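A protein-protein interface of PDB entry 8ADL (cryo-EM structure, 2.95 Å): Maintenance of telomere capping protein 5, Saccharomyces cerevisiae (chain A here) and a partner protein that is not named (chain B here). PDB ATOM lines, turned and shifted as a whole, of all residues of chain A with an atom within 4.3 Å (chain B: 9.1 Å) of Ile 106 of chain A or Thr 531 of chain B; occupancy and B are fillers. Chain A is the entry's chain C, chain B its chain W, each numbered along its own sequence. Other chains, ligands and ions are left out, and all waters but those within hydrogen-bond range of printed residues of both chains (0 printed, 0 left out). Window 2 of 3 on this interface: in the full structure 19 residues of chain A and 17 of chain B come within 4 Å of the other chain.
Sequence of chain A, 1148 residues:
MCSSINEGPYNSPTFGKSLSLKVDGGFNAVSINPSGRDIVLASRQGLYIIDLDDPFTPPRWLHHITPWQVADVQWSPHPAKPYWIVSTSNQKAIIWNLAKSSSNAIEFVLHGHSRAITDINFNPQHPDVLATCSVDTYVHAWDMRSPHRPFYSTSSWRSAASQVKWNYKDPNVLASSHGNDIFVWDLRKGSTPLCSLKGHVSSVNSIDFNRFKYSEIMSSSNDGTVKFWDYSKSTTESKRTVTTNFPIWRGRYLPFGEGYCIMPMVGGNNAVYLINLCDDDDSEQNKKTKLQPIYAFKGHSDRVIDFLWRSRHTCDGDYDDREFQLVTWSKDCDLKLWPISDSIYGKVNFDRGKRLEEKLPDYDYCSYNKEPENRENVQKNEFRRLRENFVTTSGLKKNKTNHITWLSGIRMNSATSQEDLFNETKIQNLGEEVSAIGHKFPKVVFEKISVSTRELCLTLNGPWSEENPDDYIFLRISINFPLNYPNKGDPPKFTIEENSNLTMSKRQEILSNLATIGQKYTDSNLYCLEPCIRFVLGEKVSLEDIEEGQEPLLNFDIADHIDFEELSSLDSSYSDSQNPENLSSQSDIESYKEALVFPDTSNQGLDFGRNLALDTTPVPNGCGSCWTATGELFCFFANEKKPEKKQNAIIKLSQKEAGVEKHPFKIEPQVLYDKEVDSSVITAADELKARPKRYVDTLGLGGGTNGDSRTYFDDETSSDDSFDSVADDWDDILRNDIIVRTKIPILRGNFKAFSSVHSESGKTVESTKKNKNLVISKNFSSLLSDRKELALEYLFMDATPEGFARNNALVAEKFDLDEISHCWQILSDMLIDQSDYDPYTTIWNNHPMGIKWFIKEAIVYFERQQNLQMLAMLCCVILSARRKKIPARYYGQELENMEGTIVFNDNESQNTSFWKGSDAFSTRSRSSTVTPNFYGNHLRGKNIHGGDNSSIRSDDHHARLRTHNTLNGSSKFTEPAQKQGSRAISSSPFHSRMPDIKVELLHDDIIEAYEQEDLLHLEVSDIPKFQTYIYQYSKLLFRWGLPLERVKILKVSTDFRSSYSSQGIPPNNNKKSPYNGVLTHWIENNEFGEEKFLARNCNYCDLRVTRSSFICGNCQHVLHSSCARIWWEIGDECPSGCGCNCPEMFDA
O of Asp 524 of chain B lies within hydrogen-bond range of N of Gly 529 of chain B.
NZ of Lys 92 of chain A sits at hydrogen-bond distance from O of Met 528 of chain B.
The side-chain amide oxygen (OD1) of Asn 104 of chain A is in hydrogen-bond range of the side-chain amide nitrogen (ND2) of Asn 533 of chain B (2.6 Å).
Of the 12 printed residues of chain A, 5 touch a printed residue of chain B.
Of the 12 printed residues of chain B, 4 touch a printed residue of chain A.
Printed residues of chain B that touch a printed residue of chain A: Met 528, Gly 529, Thr 531 and Asn 533.
Along chain B the printed residues that touch a printed residue of chain A span positions 528 to 533.
Gly 529 of chain B touches Lys 92 of chain A.
Lys 92 of chain A touches Thr 531 of chain B (CE to OG1, 3.3 Å).
Ile 94 of chain A touches Thr 531 of chain B (CD1 to CG2, 3.8 Å).
Thr 531 of chain B touches Ile 106 of chain A.
Asn 533 of chain B touches Ile 106 of chain A (ND2 to CD1, 3.4 Å).
OG1 of Thr 531 of chain B touches CG2 of Val 109 of chain A, 3.3 Å away.
Of the printed residues of chain B, Ile 106 of chain A touches Thr 531 and Asn 533.
Thr 531 of chain B touches just these residues of chain A: Lys 92, Ile 94, Ile 106 and Val 109.
No residue of chain B comes within 4 Å of Ala 105 of chain A.
Printed residues of chain B within 4 Å of Ile 94 of chain A: Thr 531 (3.8 Å).
Printed residues of chain A within 4 Å of Asn 533 of chain B: Asn 104 and Ile 106.
The nearest printed residue of chain A that does not touch Thr 531 of chain B is His 64 of chain A (4.3 Å).
The nearest printed residue of chain A that does not touch Gly 529 of chain B is Val 109 of chain A (6.2 Å).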
ATOM      1  N   HIS A  64       4.414   9.439 -24.809  1.00  0.00           N
ATOM      2  CA  HIS A  64       5.095   8.265 -24.268  1.00  0.00           C
ATOM      3  C   HIS A  64       5.363   8.527 -22.793  1.00  0.00           C
ATOM      4  O   HIS A  64       6.242   9.324 -22.457  1.00  0.00           O
ATOM      5  CB  HIS A  64       6.393   7.975 -25.016  1.00  0.00           C
ATOM      6  CG  HIS A  64       7.101   6.747 -24.535  1.00  0.00           C
ATOM      7  ND1 HIS A  64       6.576   5.481 -24.682  1.00  0.00           N
ATOM      8  CD2 HIS A  64       8.288   6.592 -23.904  1.00  0.00           C
ATOM      9  CE1 HIS A  64       7.411   4.598 -24.165  1.00  0.00           C
ATOM     10  NE2 HIS A  64       8.458   5.246 -23.686  1.00  0.00           N
ATOM     11  N   LYS A  92      15.625   1.260 -23.245  1.00  0.00           N
ATOM     12  CA  LYS A  92      15.393   1.009 -24.659  1.00  0.00           C
ATOM     13  C   LYS A  92      15.342   2.333 -25.412  1.00  0.00           C
ATOM     14  O   LYS A  92      14.924   3.359 -24.870  1.00  0.00           O
ATOM     15  CB  LYS A  92      14.099   0.209 -24.885  1.00  0.00           C
ATOM     16  CG  LYS A  92      12.853   0.854 -24.306  1.00  0.00           C
ATOM     17  CD  LYS A  92      11.834  -0.190 -23.883  1.00  0.00           C
ATOM     18  CE  LYS A  92      10.526   0.459 -23.464  1.00  0.00           C
ATOM     19  NZ  LYS A  92      10.717   1.397 -22.324  1.00  0.00           N
ATOM     20  N   ILE A  94      13.887   4.476 -28.654  1.00  0.00           N
ATOM     21  CA  ILE A  94      12.656   4.503 -29.433  1.00  0.00           C
ATOM     22  C   ILE A  94      12.888   5.352 -30.676  1.00  0.00           C
ATOM     23  O   ILE A  94      13.276   6.522 -30.576  1.00  0.00           O
ATOM     24  CB  ILE A  94      11.482   5.045 -28.605  1.00  0.00           C
ATOM     25  CG1 ILE A  94      11.074   4.028 -27.535  1.00  0.00           C
ATOM     26  CG2 ILE A  94      10.309   5.398 -29.503  1.00  0.00           C
ATOM     27  CD1 ILE A  94       9.821   4.404 -26.776  1.00  0.00           C
ATOM     28  N   ILE A  95      12.656   4.761 -31.845  1.00  0.00           N
ATOM     29  CA  ILE A  95      12.747   5.458 -33.124  1.00  0.00           C
ATOM     30  C   ILE A  95      11.353   5.926 -33.523  1.00  0.00           C
ATOM     31  O   ILE A  95      10.447   5.107 -33.724  1.00  0.00           O
ATOM     32  CB  ILE A  95      13.388   4.583 -34.216  1.00  0.00           C
ATOM     33  CG1 ILE A  95      14.859   4.283 -33.890  1.00  0.00           C
ATOM     34  CG2 ILE A  95      13.279   5.262 -35.573  1.00  0.00           C
ATOM     35  CD1 ILE A  95      15.121   3.032 -33.075  1.00  0.00           C
ATOM     36  N   TRP A  96      11.181   7.241 -33.645  1.00  0.00           N
ATOM     37  CA  TRP A  96       9.888   7.844 -33.942  1.00  0.00           C
ATOM     38  C   TRP A  96       9.761   8.127 -35.435  1.00  0.00           C
ATOM     39  O   TRP A  96      10.701   8.619 -36.066  1.00  0.00           O
ATOM     40  CB  TRP A  96       9.704   9.148 -33.164  1.00  0.00           C
ATOM     41  CG  TRP A  96       9.787   9.004 -31.674  1.00  0.00           C
ATOM     42  CD1 TRP A  96      10.921   8.937 -30.919  1.00  0.00           C
ATOM     43  CD2 TRP A  96       8.690   8.935 -30.756  1.00  0.00           C
ATOM     44  NE1 TRP A  96      10.600   8.819 -29.589  1.00  0.00           N
ATOM     45  CE2 TRP A  96       9.236   8.816 -29.462  1.00  0.00           C
ATOM     46  CE3 TRP A  96       7.300   8.955 -30.902  1.00  0.00           C
ATOM     47  CZ2 TRP A  96       8.440   8.718 -28.321  1.00  0.00           C
ATOM     48  CZ3 TRP A  96       6.512   8.859 -29.769  1.00  0.00           C
ATOM     49  CH2 TRP A  96       7.083   8.741 -28.496  1.00  0.00           C
ATOM     50  N   LYS A 100       4.043   8.989 -39.531  1.00  0.00           N
ATOM     51  CA  LYS A 100       2.941   8.314 -38.869  1.00  0.00           C
ATOM     52  C   LYS A 100       2.147   9.309 -38.028  1.00  0.00           C
ATOM     53  O   LYS A 100       2.599  10.420 -37.737  1.00  0.00           O
ATOM     54  CB  LYS A 100       3.460   7.182 -37.983  1.00  0.00           C
ATOM     55  CG  LYS A 100       3.844   5.920 -38.732  1.00  0.00           C
ATOM     56  CD  LYS A 100       4.215   4.810 -37.764  1.00  0.00           C
ATOM     57  CE  LYS A 100       4.640   3.551 -38.499  1.00  0.00           C
ATOM     58  NZ  LYS A 100       4.919   2.430 -37.558  1.00  0.00           N
ATOM     59  N   ASN A 104       0.213   6.728 -32.863  1.00  0.00           N
ATOM     60  CA  ASN A 104       1.212   5.666 -33.002  1.00  0.00           C
ATOM     61  C   ASN A 104       2.305   6.164 -33.945  1.00  0.00           C
ATOM     62  O   ASN A 104       2.245   5.937 -35.156  1.00  0.00           O
ATOM     63  CB  ASN A 104       0.574   4.374 -33.505  1.00  0.00           C
ATOM     64  CG  ASN A 104       1.346   3.141 -33.079  1.00  0.00           C
ATOM     65  OD1 ASN A 104       2.431   3.241 -32.507  1.00  0.00           O
ATOM     66  ND2 ASN A 104       0.788   1.967 -33.353  1.00  0.00           N
ATOM     67  N   ALA A 105       3.305   6.839 -33.380  1.00  0.00           N
ATOM     68  CA  ALA A 105       4.431   7.372 -34.135  1.00  0.00           C
ATOM     69  C   ALA A 105       5.707   6.559 -33.968  1.00  0.00           C
ATOM     70  O   ALA A 105       6.722   6.894 -34.587  1.00  0.00           O
ATOM     71  CB  ALA A 105       4.692   8.828 -33.733  1.00  0.00           C
ATOM     72  N   ILE A 106       5.686   5.506 -33.157  1.00  0.00           N
ATOM     73  CA  ILE A 106       6.877   4.698 -32.912  1.00  0.00           C
ATOM     74  C   ILE A 106       7.014   3.668 -34.027  1.00  0.00           C
ATOM     75  O   ILE A 106       6.089   2.891 -34.288  1.00  0.00           O
ATOM     76  CB  ILE A 106       6.811   4.024 -31.535  1.00  0.00           C
ATOM     77  CG1 ILE A 106       6.759   5.091 -30.437  1.00  0.00           C
ATOM     78  CG2 ILE A 106       7.995   3.088 -31.337  1.00  0.00           C
ATOM     79  CD1 ILE A 106       6.660   4.536 -29.037  1.00  0.00           C
ATOM     80  N   GLU A 107       8.172   3.662 -34.688  1.00  0.00           N
ATOM     81  CA  GLU A 107       8.441   2.727 -35.777  1.00  0.00           C
ATOM     82  C   GLU A 107       9.037   1.413 -35.274  1.00  0.00           C
ATOM     83  O   GLU A 107       8.459   0.342 -35.485  1.00  0.00           O
ATOM     84  CB  GLU A 107       9.374   3.388 -36.800  1.00  0.00           C
ATOM     85  CG  GLU A 107       9.317   2.778 -38.188  1.00  0.00           C
ATOM     86  CD  GLU A 107       9.982   3.655 -39.230  1.00  0.00           C
ATOM     87  OE1 GLU A 107      10.421   4.770 -38.878  1.00  0.00           O
ATOM     88  OE2 GLU A 107      10.066   3.230 -40.401  1.00  0.00           O
ATOM     89  N   PHE A 108      10.189   1.478 -34.609  1.00  0.00           N
ATOM     90  CA  PHE A 108      10.787   0.298 -33.997  1.00  0.00           C
ATOM     91  C   PHE A 108      11.603   0.717 -32.781  1.00  0.00           C
ATOM     92  O   PHE A 108      12.017   1.872 -32.654  1.00  0.00           O
ATOM     93  CB  PHE A 108      11.660  -0.484 -34.993  1.00  0.00           C
ATOM     94  CG  PHE A 108      12.476   0.387 -35.910  1.00  0.00           C
ATOM     95  CD1 PHE A 108      13.717   0.858 -35.521  1.00  0.00           C
ATOM     96  CD2 PHE A 108      12.016   0.703 -37.180  1.00  0.00           C
ATOM     97  CE1 PHE A 108      14.471   1.657 -36.367  1.00  0.00           C
ATOM     98  CE2 PHE A 108      12.765   1.497 -38.030  1.00  0.00           C
ATOM     99  CZ  PHE A 108      13.994   1.973 -37.623  1.00  0.00           C
ATOM    100  N   VAL A 109      11.822  -0.242 -31.882  1.00  0.00           N
ATOM    101  CA  VAL A 109      12.482  -0.005 -30.602  1.00  0.00           C
ATOM    102  C   VAL A 109      13.712  -0.897 -30.507  1.00  0.00           C
ATOM    103  O   VAL A 109      13.632  -2.104 -30.766  1.00  0.00           O
ATOM    104  CB  VAL A 109      11.528  -0.267 -29.419  1.00  0.00           C
ATOM    105  CG1 VAL A 109      12.198   0.081 -28.100  1.00  0.00           C
ATOM    106  CG2 VAL A 109      10.239   0.525 -29.588  1.00  0.00           C
ATOM    107  N   ASP B 524       9.230  -7.780 -17.299  1.00  0.00           N
ATOM    108  CA  ASP B 524       9.031  -6.863 -18.413  1.00  0.00           C
ATOM    109  C   ASP B 524       8.049  -5.748 -18.081  1.00  0.00           C
ATOM    110  O   ASP B 524       8.043  -4.723 -18.771  1.00  0.00           O
ATOM    111  CB  ASP B 524       8.554  -7.628 -19.645  1.00  0.00           C
ATOM    112  CG  ASP B 524       9.637  -8.498 -20.245  1.00  0.00           C
ATOM    113  OD1 ASP B 524      10.729  -8.590 -19.647  1.00  0.00           O
ATOM    114  OD2 ASP B 524       9.395  -9.094 -21.315  1.00  0.00           O
ATOM    115  N   LEU B 525       7.221  -5.919 -17.051  1.00  0.00           N
ATOM    116  CA  LEU B 525       6.323  -4.855 -16.616  1.00  0.00           C
ATOM    117  C   LEU B 525       6.873  -4.051 -15.449  1.00  0.00           C
ATOM    118  O   LEU B 525       6.556  -2.863 -15.329  1.00  0.00           O
ATOM    119  CB  LEU B 525       4.950  -5.425 -16.241  1.00  0.00           C
ATOM    120  CG  LEU B 525       4.083  -5.854 -17.428  1.00  0.00           C
ATOM    121  CD1 LEU B 525       2.882  -6.671 -16.976  1.00  0.00           C
ATOM    122  CD2 LEU B 525       3.641  -4.637 -18.223  1.00  0.00           C
ATOM    123  N   MET B 527      10.219  -3.524 -15.056  1.00  0.00           N
ATOM    124  CA  MET B 527      11.255  -2.736 -15.710  1.00  0.00           C
ATOM    125  C   MET B 527      10.730  -1.925 -16.885  1.00  0.00           C
ATOM    126  O   MET B 527      11.503  -1.146 -17.456  1.00  0.00           O
ATOM    127  CB  MET B 527      12.395  -3.640 -16.185  1.00  0.00           C
ATOM    128  CG  MET B 527      13.057  -4.438 -15.078  1.00  0.00           C
ATOM    129  SD  MET B 527      14.030  -3.399 -13.973  1.00  0.00           S
ATOM    130  CE  MET B 527      15.604  -3.368 -14.826  1.00  0.00           C
ATOM    131  N   MET B 528       9.449  -2.094 -17.242  1.00  0.00           N
ATOM    132  CA  MET B 528       8.823  -1.463 -18.413  1.00  0.00           C
ATOM    133  C   MET B 528       9.607  -1.758 -19.690  1.00  0.00           C
ATOM    134  O   MET B 528       9.859  -0.872 -20.511  1.00  0.00           O
ATOM    135  CB  MET B 528       8.652   0.046 -18.209  1.00  0.00           C
ATOM    136  CG  MET B 528       7.539   0.425 -17.244  1.00  0.00           C
ATOM    137  SD  MET B 528       6.876   2.071 -17.567  1.00  0.00           S
ATOM    138  CE  MET B 528       5.705   2.239 -16.221  1.00  0.00           C
ATOM    139  N   GLY B 529       9.998  -3.020 -19.858  1.00  0.00           N
ATOM    140  CA  GLY B 529      10.830  -3.409 -20.980  1.00  0.00           C
ATOM    141  C   GLY B 529      10.127  -3.505 -22.312  1.00  0.00           C
ATOM    142  O   GLY B 529      10.800  -3.574 -23.345  1.00  0.00           O
ATOM    143  N   ILE B 530       8.799  -3.502 -22.322  1.00  0.00           N
ATOM    144  CA  ILE B 530       8.019  -3.598 -23.550  1.00  0.00           C
ATOM    145  C   ILE B 530       7.399  -2.233 -23.823  1.00  0.00           C
ATOM    146  O   ILE B 530       6.705  -1.676 -22.963  1.00  0.00           O
ATOM    147  CB  ILE B 530       6.943  -4.688 -23.458  1.00  0.00           C
ATOM    148  CG1 ILE B 530       7.514  -5.951 -22.807  1.00  0.00           C
ATOM    149  CG2 ILE B 530       6.406  -5.012 -24.840  1.00  0.00           C
ATOM    150  CD1 ILE B 530       8.571  -6.654 -23.637  1.00  0.00           C
ATOM    151  N   THR B 531       7.663  -1.697 -25.012  1.00  0.00           N
ATOM    152  CA  THR B 531       7.154  -0.387 -25.398  1.00  0.00           C
ATOM    153  C   THR B 531       5.639  -0.448 -25.575  1.00  0.00           C
ATOM    154  O   THR B 531       5.107  -1.435 -26.087  1.00  0.00           O
ATOM    155  CB  THR B 531       7.844   0.065 -26.688  1.00  0.00           C
ATOM    156  OG1 THR B 531       9.261   0.026 -26.495  1.00  0.00           O
ATOM    157  CG2 THR B 531       7.455   1.486 -27.066  1.00  0.00           C
ATOM    158  N   GLU B 532       4.952   0.628 -25.159  1.00  0.00           N
ATOM    159  CA  GLU B 532       3.493   0.632 -25.033  1.00  0.00           C
ATOM    160  C   GLU B 532       2.777   0.357 -26.355  1.00  0.00           C
ATOM    161  O   GLU B 532       1.669  -0.193 -26.354  1.00  0.00           O
ATOM    162  CB  GLU B 532       3.031   1.971 -24.452  1.00  0.00           C
ATOM    163  CG  GLU B 532       1.613   1.969 -23.902  1.00  0.00           C
ATOM    164  CD  GLU B 532       1.222   3.299 -23.288  1.00  0.00           C
ATOM    165  OE1 GLU B 532       2.012   4.261 -23.397  1.00  0.00           O
ATOM    166  OE2 GLU B 532       0.125   3.383 -22.697  1.00  0.00           O
ATOM    167  N   ASN B 533       3.388   0.708 -27.484  1.00  0.00           N
ATOM    168  CA  ASN B 533       2.750   0.490 -28.775  1.00  0.00           C
ATOM    169  C   ASN B 533       2.877  -0.941 -29.285  1.00  0.00           C
ATOM    170  O   ASN B 533       2.242  -1.272 -30.292  1.00  0.00           O
ATOM    171  CB  ASN B 533       3.313   1.456 -29.820  1.00  0.00           C
ATOM    172  CG  ASN B 533       3.184   2.905 -29.399  1.00  0.00           C
ATOM    173  OD1 ASN B 533       2.698   3.206 -28.309  1.00  0.00           O
ATOM    174  ND2 ASN B 533       3.593   3.814 -30.275  1.00  0.00           N
ATOM    175  N   GLU B 534       3.672  -1.795 -28.637  1.00  0.00           N
ATOM    176  CA  GLU B 534       3.935  -3.125 -29.169  1.00  0.00           C
ATOM    177  C   GLU B 534       3.464  -4.265 -28.272  1.00  0.00           C
ATOM    178  O   GLU B 534       3.665  -5.429 -28.636  1.00  0.00           O
ATOM    179  CB  GLU B 534       5.432  -3.295 -29.476  1.00  0.00           C
ATOM    180  CG  GLU B 534       6.320  -3.498 -28.262  1.00  0.00           C
ATOM    181  CD  GLU B 534       7.720  -3.946 -28.634  1.00  0.00           C
ATOM    182  OE1 GLU B 534       7.955  -4.242 -29.824  1.00  0.00           O
ATOM    183  OE2 GLU B 534       8.585  -4.001 -27.735  1.00  0.00           O
ATOM    184  N   LEU B 535       2.839  -3.983 -27.128  1.00  0.00           N
ATOM    185  CA  LEU B 535       2.167  -5.025 -26.358  1.00  0.00           C
ATOM    186  C   LEU B 535       0.659  -4.807 -26.317  1.00  0.00           C
ATOM    187  O   LEU B 535      -0.019  -5.330 -25.427  1.00  0.00           O
ATOM    188  CB  LEU B 535       2.730  -5.142 -24.934  1.00  0.00           C
ATOM    189  CG  LEU B 535       2.490  -4.168 -23.771  1.00  0.00           C
ATOM    190  CD1 LEU B 535       2.898  -4.827 -22.463  1.00  0.00           C
ATOM    191  CD2 LEU B 535       3.223  -2.873 -23.930  1.00  0.00           C
ATOM    192  N   ILE B 536       0.128  -4.040 -27.274  1.00  0.00           N
ATOM    193  CA  ILE B 536      -1.314  -3.857 -27.389  1.00  0.00           C
ATOM    194  C   ILE B 536      -1.967  -5.201 -27.682  1.00  0.00           C
ATOM    195  O   ILE B 536      -1.426  -6.025 -28.431  1.00  0.00           O
ATOM    196  CB  ILE B 536      -1.613  -2.817 -28.485  1.00  0.00           C
ATOM    197  CG1 ILE B 536      -0.953  -1.479 -28.142  1.00  0.00           C
ATOM    198  CG2 ILE B 536      -3.113  -2.610 -28.683  1.00  0.00           C
ATOM    199  CD1 ILE B 536      -1.566  -0.780 -26.946  1.00  0.00           C
